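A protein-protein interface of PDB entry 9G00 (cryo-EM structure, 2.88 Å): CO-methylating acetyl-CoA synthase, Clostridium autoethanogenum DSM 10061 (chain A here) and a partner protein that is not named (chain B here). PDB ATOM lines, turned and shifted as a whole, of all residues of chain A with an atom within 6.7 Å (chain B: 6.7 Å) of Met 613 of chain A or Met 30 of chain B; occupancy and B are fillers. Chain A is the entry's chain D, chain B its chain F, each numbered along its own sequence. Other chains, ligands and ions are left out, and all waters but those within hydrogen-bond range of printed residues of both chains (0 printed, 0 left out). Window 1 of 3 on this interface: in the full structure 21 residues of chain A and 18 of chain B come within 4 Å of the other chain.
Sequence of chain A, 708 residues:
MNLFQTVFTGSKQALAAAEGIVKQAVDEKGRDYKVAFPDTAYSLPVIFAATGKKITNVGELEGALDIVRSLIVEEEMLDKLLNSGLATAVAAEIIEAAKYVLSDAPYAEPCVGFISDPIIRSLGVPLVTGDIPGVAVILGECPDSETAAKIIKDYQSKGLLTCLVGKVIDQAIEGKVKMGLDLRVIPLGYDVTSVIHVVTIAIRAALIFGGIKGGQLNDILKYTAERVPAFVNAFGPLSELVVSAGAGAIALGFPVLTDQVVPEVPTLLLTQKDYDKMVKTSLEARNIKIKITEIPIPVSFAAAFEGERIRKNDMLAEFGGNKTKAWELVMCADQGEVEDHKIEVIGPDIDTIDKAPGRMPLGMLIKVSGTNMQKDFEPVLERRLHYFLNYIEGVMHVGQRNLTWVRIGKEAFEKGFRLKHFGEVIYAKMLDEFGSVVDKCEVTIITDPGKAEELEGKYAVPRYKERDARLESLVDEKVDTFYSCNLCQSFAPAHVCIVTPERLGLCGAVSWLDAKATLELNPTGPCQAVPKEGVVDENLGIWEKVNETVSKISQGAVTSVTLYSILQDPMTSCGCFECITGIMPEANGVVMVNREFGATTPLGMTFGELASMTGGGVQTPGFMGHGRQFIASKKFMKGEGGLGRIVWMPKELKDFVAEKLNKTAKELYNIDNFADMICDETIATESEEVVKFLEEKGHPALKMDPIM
Of the 17 printed residues of chain B, 4 touch a printed residue of chain A.
Hydrophobic or aromatic side chains of chain B within 4 Å of the printed part of chain A: Leu 6, Leu 26 and Met 30.
Of the 16 printed residues of chain A, 4 touch a printed residue of chain B.
Hydrophobic or aromatic side chains of chain A within 4 Å of the printed part of chain B: Met 605, Met 613 and Phe 623.
Among the printed residues, 5 pairs touch across the chains.
Among the printed residues, no Asp or Glu carboxylate lies within 4 Å of a Lys or Arg side-chain nitrogen of the other chain.
Met 605 of chain A touches Ala 27 of chain B.
Met 30 of chain B touches Met 613 of chain A (CE to CE, 3.6 Å).
Pro 621 of chain A touches Leu 6 of chain B (O to CD1, 3.4 Å).
Phe 623 of chain A touches Leu 26 of chain B.
Met 30 of chain B touches Phe 623 of chain A.
O of Phe 623 of chain A lies within hydrogen-bond range of OG1 of Thr 620 of chain A (3.5 Å).
Of chain A, only Met 613 (3.6 Å) and Phe 623 (3.6 Å) come within 4 Å of Met 30 of chain B.
Printed residues of chain B within 4 Å of Pro 621 of chain A: Leu 6 (3.4 Å).
Printed residues of chain B within 4 Å of Phe 623 of chain A: Leu 26 and Met 30.
Printed residues of chain A within 4 Å of Ala 27 of chain B: Met 605 (3.997 Å).
Printed residues of chain A within 4 Å of Leu 26 of chain B: Phe 623 (3.8 Å).
Of the printed residues of chain B, Met 605 of chain A touches Ala 27.
The nearest residue of chain A that does not touch Met 30 of chain B is Met 605 of chain A (4.5 Å).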
ATOM      1  N   ILE A 580       2.584 -31.781 -12.036  1.00  0.00           N
ATOM      2  CA  ILE A 580       1.634 -30.682 -12.132  1.00  0.00           C
ATOM      3  C   ILE A 580       0.499 -30.966 -11.163  1.00  0.00           C
ATOM      4  O   ILE A 580      -0.041 -32.077 -11.143  1.00  0.00           O
ATOM      5  CB  ILE A 580       1.098 -30.511 -13.566  1.00  0.00           C
ATOM      6  CG1 ILE A 580      -0.092 -29.553 -13.573  1.00  0.00           C
ATOM      7  CG2 ILE A 580       0.713 -31.856 -14.152  1.00  0.00           C
ATOM      8  CD1 ILE A 580      -0.673 -29.334 -14.919  1.00  0.00           C
ATOM      9  N   MET A 605      -8.324 -35.485 -16.977  1.00  0.00           N
ATOM     10  CA  MET A 605      -7.303 -35.103 -17.937  1.00  0.00           C
ATOM     11  C   MET A 605      -5.986 -35.755 -17.549  1.00  0.00           C
ATOM     12  O   MET A 605      -5.658 -35.850 -16.363  1.00  0.00           O
ATOM     13  CB  MET A 605      -7.150 -33.582 -17.991  1.00  0.00           C
ATOM     14  CG  MET A 605      -8.393 -32.866 -18.491  1.00  0.00           C
ATOM     15  SD  MET A 605      -8.417 -31.111 -18.078  1.00  0.00           S
ATOM     16  CE  MET A 605      -8.769 -31.175 -16.324  1.00  0.00           C
ATOM     17  N   GLY A 608      -0.445 -35.055 -20.293  1.00  0.00           N
ATOM     18  CA  GLY A 608      -0.302 -34.334 -21.547  1.00  0.00           C
ATOM     19  C   GLY A 608      -1.402 -33.312 -21.756  1.00  0.00           C
ATOM     20  O   GLY A 608      -1.149 -32.200 -22.224  1.00  0.00           O
ATOM     21  N   GLU A 609      -2.639 -33.679 -21.423  1.00  0.00           N
ATOM     22  CA  GLU A 609      -3.745 -32.739 -21.566  1.00  0.00           C
ATOM     23  C   GLU A 609      -3.587 -31.558 -20.619  1.00  0.00           C
ATOM     24  O   GLU A 609      -3.841 -30.410 -21.001  1.00  0.00           O
ATOM     25  CB  GLU A 609      -5.071 -33.452 -21.314  1.00  0.00           C
ATOM     26  CG  GLU A 609      -5.243 -34.731 -22.116  1.00  0.00           C
ATOM     27  CD  GLU A 609      -6.549 -35.432 -21.818  1.00  0.00           C
ATOM     28  OE1 GLU A 609      -7.591 -34.748 -21.751  1.00  0.00           O
ATOM     29  OE2 GLU A 609      -6.531 -36.667 -21.642  1.00  0.00           O
ATOM     30  N   LEU A 610      -3.173 -31.817 -19.379  1.00  0.00           N
ATOM     31  CA  LEU A 610      -2.979 -30.732 -18.425  1.00  0.00           C
ATOM     32  C   LEU A 610      -1.782 -29.869 -18.808  1.00  0.00           C
ATOM     33  O   LEU A 610      -1.815 -28.645 -18.641  1.00  0.00           O
ATOM     34  CB  LEU A 610      -2.807 -31.294 -17.016  1.00  0.00           C
ATOM     35  CG  LEU A 610      -4.029 -31.941 -16.366  1.00  0.00           C
ATOM     36  CD1 LEU A 610      -3.640 -32.654 -15.083  1.00  0.00           C
ATOM     37  CD2 LEU A 610      -5.087 -30.896 -16.084  1.00  0.00           C
ATOM     38  N   ALA A 611      -0.724 -30.483 -19.338  1.00  0.00           N
ATOM     39  CA  ALA A 611       0.461 -29.724 -19.719  1.00  0.00           C
ATOM     40  C   ALA A 611       0.208 -28.805 -20.907  1.00  0.00           C
ATOM     41  O   ALA A 611       0.977 -27.862 -21.114  1.00  0.00           O
ATOM     42  CB  ALA A 611       1.611 -30.676 -20.041  1.00  0.00           C
ATOM     43  N   SER A 612      -0.844 -29.054 -21.688  1.00  0.00           N
ATOM     44  CA  SER A 612      -1.127 -28.213 -22.846  1.00  0.00           C
ATOM     45  C   SER A 612      -1.703 -26.861 -22.450  1.00  0.00           C
ATOM     46  O   SER A 612      -1.692 -25.935 -23.268  1.00  0.00           O
ATOM     47  CB  SER A 612      -2.090 -28.924 -23.799  1.00  0.00           C
ATOM     48  OG  SER A 612      -3.332 -29.192 -23.175  1.00  0.00           O
ATOM     49  N   MET A 613      -2.209 -26.729 -21.229  1.00  0.00           N
ATOM     50  CA  MET A 613      -2.789 -25.484 -20.738  1.00  0.00           C
ATOM     51  C   MET A 613      -1.972 -24.838 -19.631  1.00  0.00           C
ATOM     52  O   MET A 613      -1.899 -23.609 -19.565  1.00  0.00           O
ATOM     53  CB  MET A 613      -4.210 -25.732 -20.229  1.00  0.00           C
ATOM     54  CG  MET A 613      -4.357 -27.014 -19.435  1.00  0.00           C
ATOM     55  SD  MET A 613      -5.871 -27.068 -18.468  1.00  0.00           S
ATOM     56  CE  MET A 613      -5.546 -25.763 -17.288  1.00  0.00           C
ATOM     57  N   THR A 614      -1.377 -25.633 -18.742  1.00  0.00           N
ATOM     58  CA  THR A 614      -0.548 -25.063 -17.685  1.00  0.00           C
ATOM     59  C   THR A 614       0.730 -24.456 -18.247  1.00  0.00           C
ATOM     60  O   THR A 614       1.149 -23.374 -17.821  1.00  0.00           O
ATOM     61  CB  THR A 614      -0.220 -26.139 -16.651  1.00  0.00           C
ATOM     62  OG1 THR A 614      -1.411 -26.493 -15.944  1.00  0.00           O
ATOM     63  CG2 THR A 614       0.823 -25.653 -15.662  1.00  0.00           C
ATOM     64  N   GLY A 615       1.361 -25.128 -19.205  1.00  0.00           N
ATOM     65  CA  GLY A 615       2.628 -24.678 -19.732  1.00  0.00           C
ATOM     66  C   GLY A 615       2.486 -23.509 -20.683  1.00  0.00           C
ATOM     67  O   GLY A 615       1.396 -23.022 -20.977  1.00  0.00           O
ATOM     68  N   GLY A 616       3.633 -23.050 -21.171  1.00  0.00           N
ATOM     69  CA  GLY A 616       3.677 -21.952 -22.109  1.00  0.00           C
ATOM     70  C   GLY A 616       3.827 -20.583 -21.493  1.00  0.00           C
ATOM     71  O   GLY A 616       3.770 -19.588 -22.224  1.00  0.00           O
ATOM     72  N   VAL A 618       1.783 -19.070 -19.279  1.00  0.00           N
ATOM     73  CA  VAL A 618       0.504 -18.403 -19.072  1.00  0.00           C
ATOM     74  C   VAL A 618       0.074 -18.618 -17.628  1.00  0.00           C
ATOM     75  O   VAL A 618       0.359 -19.654 -17.021  1.00  0.00           O
ATOM     76  CB  VAL A 618      -0.573 -18.921 -20.049  1.00  0.00           C
ATOM     77  CG1 VAL A 618      -0.218 -18.542 -21.473  1.00  0.00           C
ATOM     78  CG2 VAL A 618      -0.730 -20.427 -19.930  1.00  0.00           C
ATOM     79  N   GLN A 619      -0.611 -17.619 -17.074  1.00  0.00           N
ATOM     80  CA  GLN A 619      -1.125 -17.689 -15.710  1.00  0.00           C
ATOM     81  C   GLN A 619      -2.491 -18.361 -15.740  1.00  0.00           C
ATOM     82  O   GLN A 619      -3.476 -17.762 -16.183  1.00  0.00           O
ATOM     83  CB  GLN A 619      -1.216 -16.299 -15.086  1.00  0.00           C
ATOM     84  CG  GLN A 619       0.092 -15.800 -14.521  1.00  0.00           C
ATOM     85  CD  GLN A 619      -0.050 -14.470 -13.825  1.00  0.00           C
ATOM     86  OE1 GLN A 619      -0.744 -13.577 -14.304  1.00  0.00           O
ATOM     87  NE2 GLN A 619       0.605 -14.330 -12.682  1.00  0.00           N
ATOM     88  N   THR A 620      -2.548 -19.605 -15.273  1.00  0.00           N
ATOM     89  CA  THR A 620      -3.790 -20.368 -15.217  1.00  0.00           C
ATOM     90  C   THR A 620      -4.146 -20.637 -13.763  1.00  0.00           C
ATOM     91  O   THR A 620      -3.549 -21.524 -13.134  1.00  0.00           O
ATOM     92  CB  THR A 620      -3.654 -21.687 -15.980  1.00  0.00           C
ATOM     93  OG1 THR A 620      -2.613 -22.473 -15.392  1.00  0.00           O
ATOM     94  CG2 THR A 620      -3.328 -21.428 -17.435  1.00  0.00           C
ATOM     95  N   PRO A 621      -5.095 -19.910 -13.180  1.00  0.00           N
ATOM     96  CA  PRO A 621      -5.475 -20.189 -11.794  1.00  0.00           C
ATOM     97  C   PRO A 621      -5.977 -21.613 -11.632  1.00  0.00           C
ATOM     98  O   PRO A 621      -6.672 -22.152 -12.495  1.00  0.00           O
ATOM     99  CB  PRO A 621      -6.583 -19.167 -11.521  1.00  0.00           C
ATOM    100  CG  PRO A 621      -6.333 -18.078 -12.488  1.00  0.00           C
ATOM    101  CD  PRO A 621      -5.801 -18.736 -13.714  1.00  0.00           C
ATOM    102  N   PHE A 623      -4.176 -24.385 -11.514  1.00  0.00           N
ATOM    103  CA  PHE A 623      -3.236 -25.382 -11.999  1.00  0.00           C
ATOM    104  C   PHE A 623      -1.830 -24.815 -11.926  1.00  0.00           C
ATOM    105  O   PHE A 623      -1.602 -23.651 -12.264  1.00  0.00           O
ATOM    106  CB  PHE A 623      -3.566 -25.804 -13.428  1.00  0.00           C
ATOM    107  CG  PHE A 623      -4.896 -26.474 -13.559  1.00  0.00           C
ATOM    108  CD1 PHE A 623      -6.055 -25.730 -13.666  1.00  0.00           C
ATOM    109  CD2 PHE A 623      -4.991 -27.850 -13.562  1.00  0.00           C
ATOM    110  CE1 PHE A 623      -7.279 -26.346 -13.779  1.00  0.00           C
ATOM    111  CE2 PHE A 623      -6.211 -28.468 -13.675  1.00  0.00           C
ATOM    112  CZ  PHE A 623      -7.356 -27.716 -13.784  1.00  0.00           C
ATOM    113  N   GLY B   5     -11.156 -20.551 -17.801  1.00  0.00           N
ATOM    114  CA  GLY B   5     -11.123 -21.953 -17.294  1.00  0.00           C
ATOM    115  C   GLY B   5     -12.007 -22.155 -16.080  1.00  0.00           C
ATOM    116  O   GLY B   5     -13.156 -22.573 -16.203  1.00  0.00           O
ATOM    117  N   LEU B   6     -11.464 -21.869 -14.895  1.00  0.00           N
ATOM    118  CA  LEU B   6     -12.260 -21.920 -13.675  1.00  0.00           C
ATOM    119  C   LEU B   6     -13.333 -20.844 -13.640  1.00  0.00           C
ATOM    120  O   LEU B   6     -14.239 -20.924 -12.805  1.00  0.00           O
ATOM    121  CB  LEU B   6     -11.365 -21.782 -12.444  1.00  0.00           C
ATOM    122  CG  LEU B   6     -10.503 -22.989 -12.072  1.00  0.00           C
ATOM    123  CD1 LEU B   6      -9.637 -22.650 -10.878  1.00  0.00           C
ATOM    124  CD2 LEU B   6     -11.352 -24.210 -11.773  1.00  0.00           C
ATOM    125  N   ASN B   7     -13.243 -19.839 -14.513  1.00  0.00           N
ATOM    126  CA  ASN B   7     -14.251 -18.787 -14.535  1.00  0.00           C
ATOM    127  C   ASN B   7     -15.616 -19.352 -14.901  1.00  0.00           C
ATOM    128  O   ASN B   7     -16.626 -19.007 -14.279  1.00  0.00           O
ATOM    129  CB  ASN B   7     -13.846 -17.698 -15.525  1.00  0.00           C
ATOM    130  CG  ASN B   7     -12.402 -17.274 -15.363  1.00  0.00           C
ATOM    131  OD1 ASN B   7     -11.579 -17.473 -16.257  1.00  0.00           O
ATOM    132  ND2 ASN B   7     -12.085 -16.691 -14.215  1.00  0.00           N
ATOM    133  N   ILE B   8     -15.665 -20.221 -15.909  1.00  0.00           N
ATOM    134  CA  ILE B   8     -16.939 -20.782 -16.331  1.00  0.00           C
ATOM    135  C   ILE B   8     -17.330 -21.995 -15.497  1.00  0.00           C
ATOM    136  O   ILE B   8     -18.496 -22.408 -15.530  1.00  0.00           O
ATOM    137  CB  ILE B   8     -16.908 -21.139 -17.826  1.00  0.00           C
ATOM    138  CG1 ILE B   8     -16.141 -22.437 -18.061  1.00  0.00           C
ATOM    139  CG2 ILE B   8     -16.321 -19.992 -18.644  1.00  0.00           C
ATOM    140  CD1 ILE B   8     -17.065 -23.597 -18.308  1.00  0.00           C
ATOM    141  N   PHE B   9     -16.391 -22.583 -14.752  1.00  0.00           N
ATOM    142  CA  PHE B   9     -16.742 -23.696 -13.875  1.00  0.00           C
ATOM    143  C   PHE B   9     -17.713 -23.255 -12.793  1.00  0.00           C
ATOM    144  O   PHE B   9     -18.512 -24.064 -12.308  1.00  0.00           O
ATOM    145  CB  PHE B   9     -15.486 -24.287 -13.236  1.00  0.00           C
ATOM    146  CG  PHE B   9     -15.729 -25.567 -12.491  1.00  0.00           C
ATOM    147  CD1 PHE B   9     -15.783 -26.776 -13.164  1.00  0.00           C
ATOM    148  CD2 PHE B   9     -15.894 -25.564 -11.120  1.00  0.00           C
ATOM    149  CE1 PHE B   9     -16.003 -27.954 -12.481  1.00  0.00           C
ATOM    150  CE2 PHE B   9     -16.115 -26.741 -10.434  1.00  0.00           C
ATOM    151  CZ  PHE B   9     -16.167 -27.936 -11.117  1.00  0.00           C
ATOM    152  N   CYS B  25     -16.824 -32.030 -15.210  1.00  0.00           N
ATOM    153  CA  CYS B  25     -17.166 -30.655 -15.550  1.00  0.00           C
ATOM    154  C   CYS B  25     -15.917 -29.793 -15.659  1.00  0.00           C
ATOM    155  O   CYS B  25     -15.851 -28.882 -16.491  1.00  0.00           O
ATOM    156  CB  CYS B  25     -18.113 -30.079 -14.498  1.00  0.00           C
ATOM    157  SG  CYS B  25     -19.753 -30.816 -14.464  1.00  0.00           S
ATOM    158  N   LEU B  26     -14.917 -30.059 -14.815  1.00  0.00           N
ATOM    159  CA  LEU B  26     -13.662 -29.323 -14.917  1.00  0.00           C
ATOM    160  C   LEU B  26     -12.973 -29.602 -16.245  1.00  0.00           C
ATOM    161  O   LEU B  26     -12.439 -28.687 -16.880  1.00  0.00           O
ATOM    162  CB  LEU B  26     -12.746 -29.684 -13.749  1.00  0.00           C
ATOM    163  CG  LEU B  26     -11.459 -28.866 -13.646  1.00  0.00           C
ATOM    164  CD1 LEU B  26     -11.767 -27.422 -13.287  1.00  0.00           C
ATOM    165  CD2 LEU B  26     -10.521 -29.486 -12.630  1.00  0.00           C
ATOM    166  N   ALA B  27     -12.980 -30.863 -16.687  1.00  0.00           N
ATOM    167  CA  ALA B  27     -12.413 -31.177 -17.994  1.00  0.00           C
ATOM    168  C   ALA B  27     -13.145 -30.426 -19.096  1.00  0.00           C
ATOM    169  O   ALA B  27     -12.519 -29.896 -20.022  1.00  0.00           O
ATOM    170  CB  ALA B  27     -12.470 -32.684 -18.244  1.00  0.00           C
ATOM    171  N   PHE B  28     -14.474 -30.364 -19.010  1.00  0.00           N
ATOM    172  CA  PHE B  28     -15.247 -29.528 -19.917  1.00  0.00           C
ATOM    173  C   PHE B  28     -15.003 -28.046 -19.673  1.00  0.00           C
ATOM    174  O   PHE B  28     -15.186 -27.241 -20.590  1.00  0.00           O
ATOM    175  CB  PHE B  28     -16.736 -29.848 -19.768  1.00  0.00           C
ATOM    176  CG  PHE B  28     -17.630 -29.026 -20.653  1.00  0.00           C
ATOM    177  CD1 PHE B  28     -17.800 -29.354 -21.985  1.00  0.00           C
ATOM    178  CD2 PHE B  28     -18.311 -27.931 -20.147  1.00  0.00           C
ATOM    179  CE1 PHE B  28     -18.624 -28.601 -22.797  1.00  0.00           C
ATOM    180  CE2 PHE B  28     -19.137 -27.176 -20.956  1.00  0.00           C
ATOM    181  CZ  PHE B  28     -19.293 -27.512 -22.281  1.00  0.00           C
ATOM    182  N   SER B  29     -14.588 -27.670 -18.465  1.00  0.00           N
ATOM    183  CA  SER B  29     -14.420 -26.257 -18.143  1.00  0.00           C
ATOM    184  C   SER B  29     -13.182 -25.669 -18.807  1.00  0.00           C
ATOM    185  O   SER B  29     -13.241 -24.588 -19.405  1.00  0.00           O
ATOM    186  CB  SER B  29     -14.356 -26.065 -16.629  1.00  0.00           C
ATOM    187  OG  SER B  29     -14.172 -24.697 -16.316  1.00  0.00           O
ATOM    188  N   MET B  30     -12.046 -26.359 -18.708  1.00  0.00           N
ATOM    189  CA  MET B  30     -10.799 -25.801 -19.219  1.00  0.00           C
ATOM    190  C   MET B  30     -10.742 -25.854 -20.737  1.00  0.00           C
ATOM    191  O   MET B  30     -10.165 -24.959 -21.367  1.00  0.00           O
ATOM    192  CB  MET B  30      -9.602 -26.545 -18.629  1.00  0.00           C
ATOM    193  CG  MET B  30      -9.714 -26.825 -17.143  1.00  0.00           C
ATOM    194  SD  MET B  30     -10.217 -25.378 -16.196  1.00  0.00           S
ATOM    195  CE  MET B  30      -8.771 -24.339 -16.358  1.00  0.00           C
ATOM    196  N   LYS B  31     -11.338 -26.879 -21.345  1.00  0.00           N
ATOM    197  CA  LYS B  31     -11.240 -27.033 -22.792  1.00  0.00           C
ATOM    198  C   LYS B  31     -12.052 -25.972 -23.526  1.00  0.00           C
ATOM    199  O   LYS B  31     -11.590 -25.423 -24.533  1.00  0.00           O
ATOM    200  CB  LYS B  31     -11.690 -28.437 -23.195  1.00  0.00           C
ATOM    201  CG  LYS B  31     -10.664 -29.528 -22.887  1.00  0.00           C
ATOM    202  CD  LYS B  31      -9.361 -29.349 -23.666  1.00  0.00           C
ATOM    203  CE  LYS B  31      -9.585 -29.385 -25.175  1.00  0.00           C
ATOM    204  NZ  LYS B  31      -8.328 -29.172 -25.944  1.00  0.00           N
ATOM    205  N   VAL B  32     -13.248 -25.647 -23.033  1.00  0.00           N
ATOM    206  CA  VAL B  32     -14.057 -24.641 -23.711  1.00  0.00           C
ATOM    207  C   VAL B  32     -13.392 -23.274 -23.629  1.00  0.00           C
ATOM    208  O   VAL B  32     -13.568 -22.438 -24.522  1.00  0.00           O
ATOM    209  CB  VAL B  32     -15.483 -24.604 -23.131  1.00  0.00           C
ATOM    210  CG1 VAL B  32     -16.137 -25.971 -23.262  1.00  0.00           C
ATOM    211  CG2 VAL B  32     -15.467 -24.139 -21.679  1.00  0.00           C
ATOM    212  N   ALA B  33     -12.627 -23.015 -22.567  1.00  0.00           N
ATOM    213  CA  ALA B  33     -11.856 -21.778 -22.510  1.00  0.00           C
ATOM    214  C   ALA B  33     -10.843 -21.726 -23.645  1.00  0.00           C
ATOM    215  O   ALA B  33     -10.612 -20.666 -24.236  1.00  0.00           O
ATOM    216  CB  ALA B  33     -11.159 -21.653 -21.156  1.00  0.00           C
ATOM    217  N   ALA B  34     -10.220 -22.865 -23.957  1.00  0.00           N
ATOM    218  CA  ALA B  34      -9.371 -22.938 -25.141  1.00  0.00           C
ATOM    219  C   ALA B  34     -10.191 -22.749 -26.411  1.00  0.00           C
ATOM    220  O   ALA B  34      -9.734 -22.107 -27.364  1.00  0.00           O
ATOM    221  CB  ALA B  34      -8.632 -24.276 -25.172  1.00  0.00           C
ATOM    222  N   GLY B  35     -11.399 -23.312 -26.447  1.00  0.00           N
ATOM    223  CA  GLY B  35     -12.309 -23.152 -27.564  1.00  0.00           C
ATOM    224  C   GLY B  35     -12.535 -24.397 -28.394  1.00  0.00           C
ATOM    225  O   GLY B  35     -13.281 -24.334 -29.377  1.00  0.00           O
ATOM    226  N   VAL B  37     -14.029 -27.596 -27.689  1.00  0.00           N
ATOM    227  CA  VAL B  37     -15.355 -28.214 -27.638  1.00  0.00           C
ATOM    228  C   VAL B  37     -16.465 -27.173 -27.757  1.00  0.00           C
ATOM    229  O   VAL B  37     -17.549 -27.481 -28.264  1.00  0.00           O
ATOM    230  CB  VAL B  37     -15.543 -29.063 -26.362  1.00  0.00           C
ATOM    231  CG1 VAL B  37     -15.390 -30.542 -26.687  1.00  0.00           C
ATOM    232  CG2 VAL B  37     -14.581 -28.659 -25.245  1.00  0.00           C
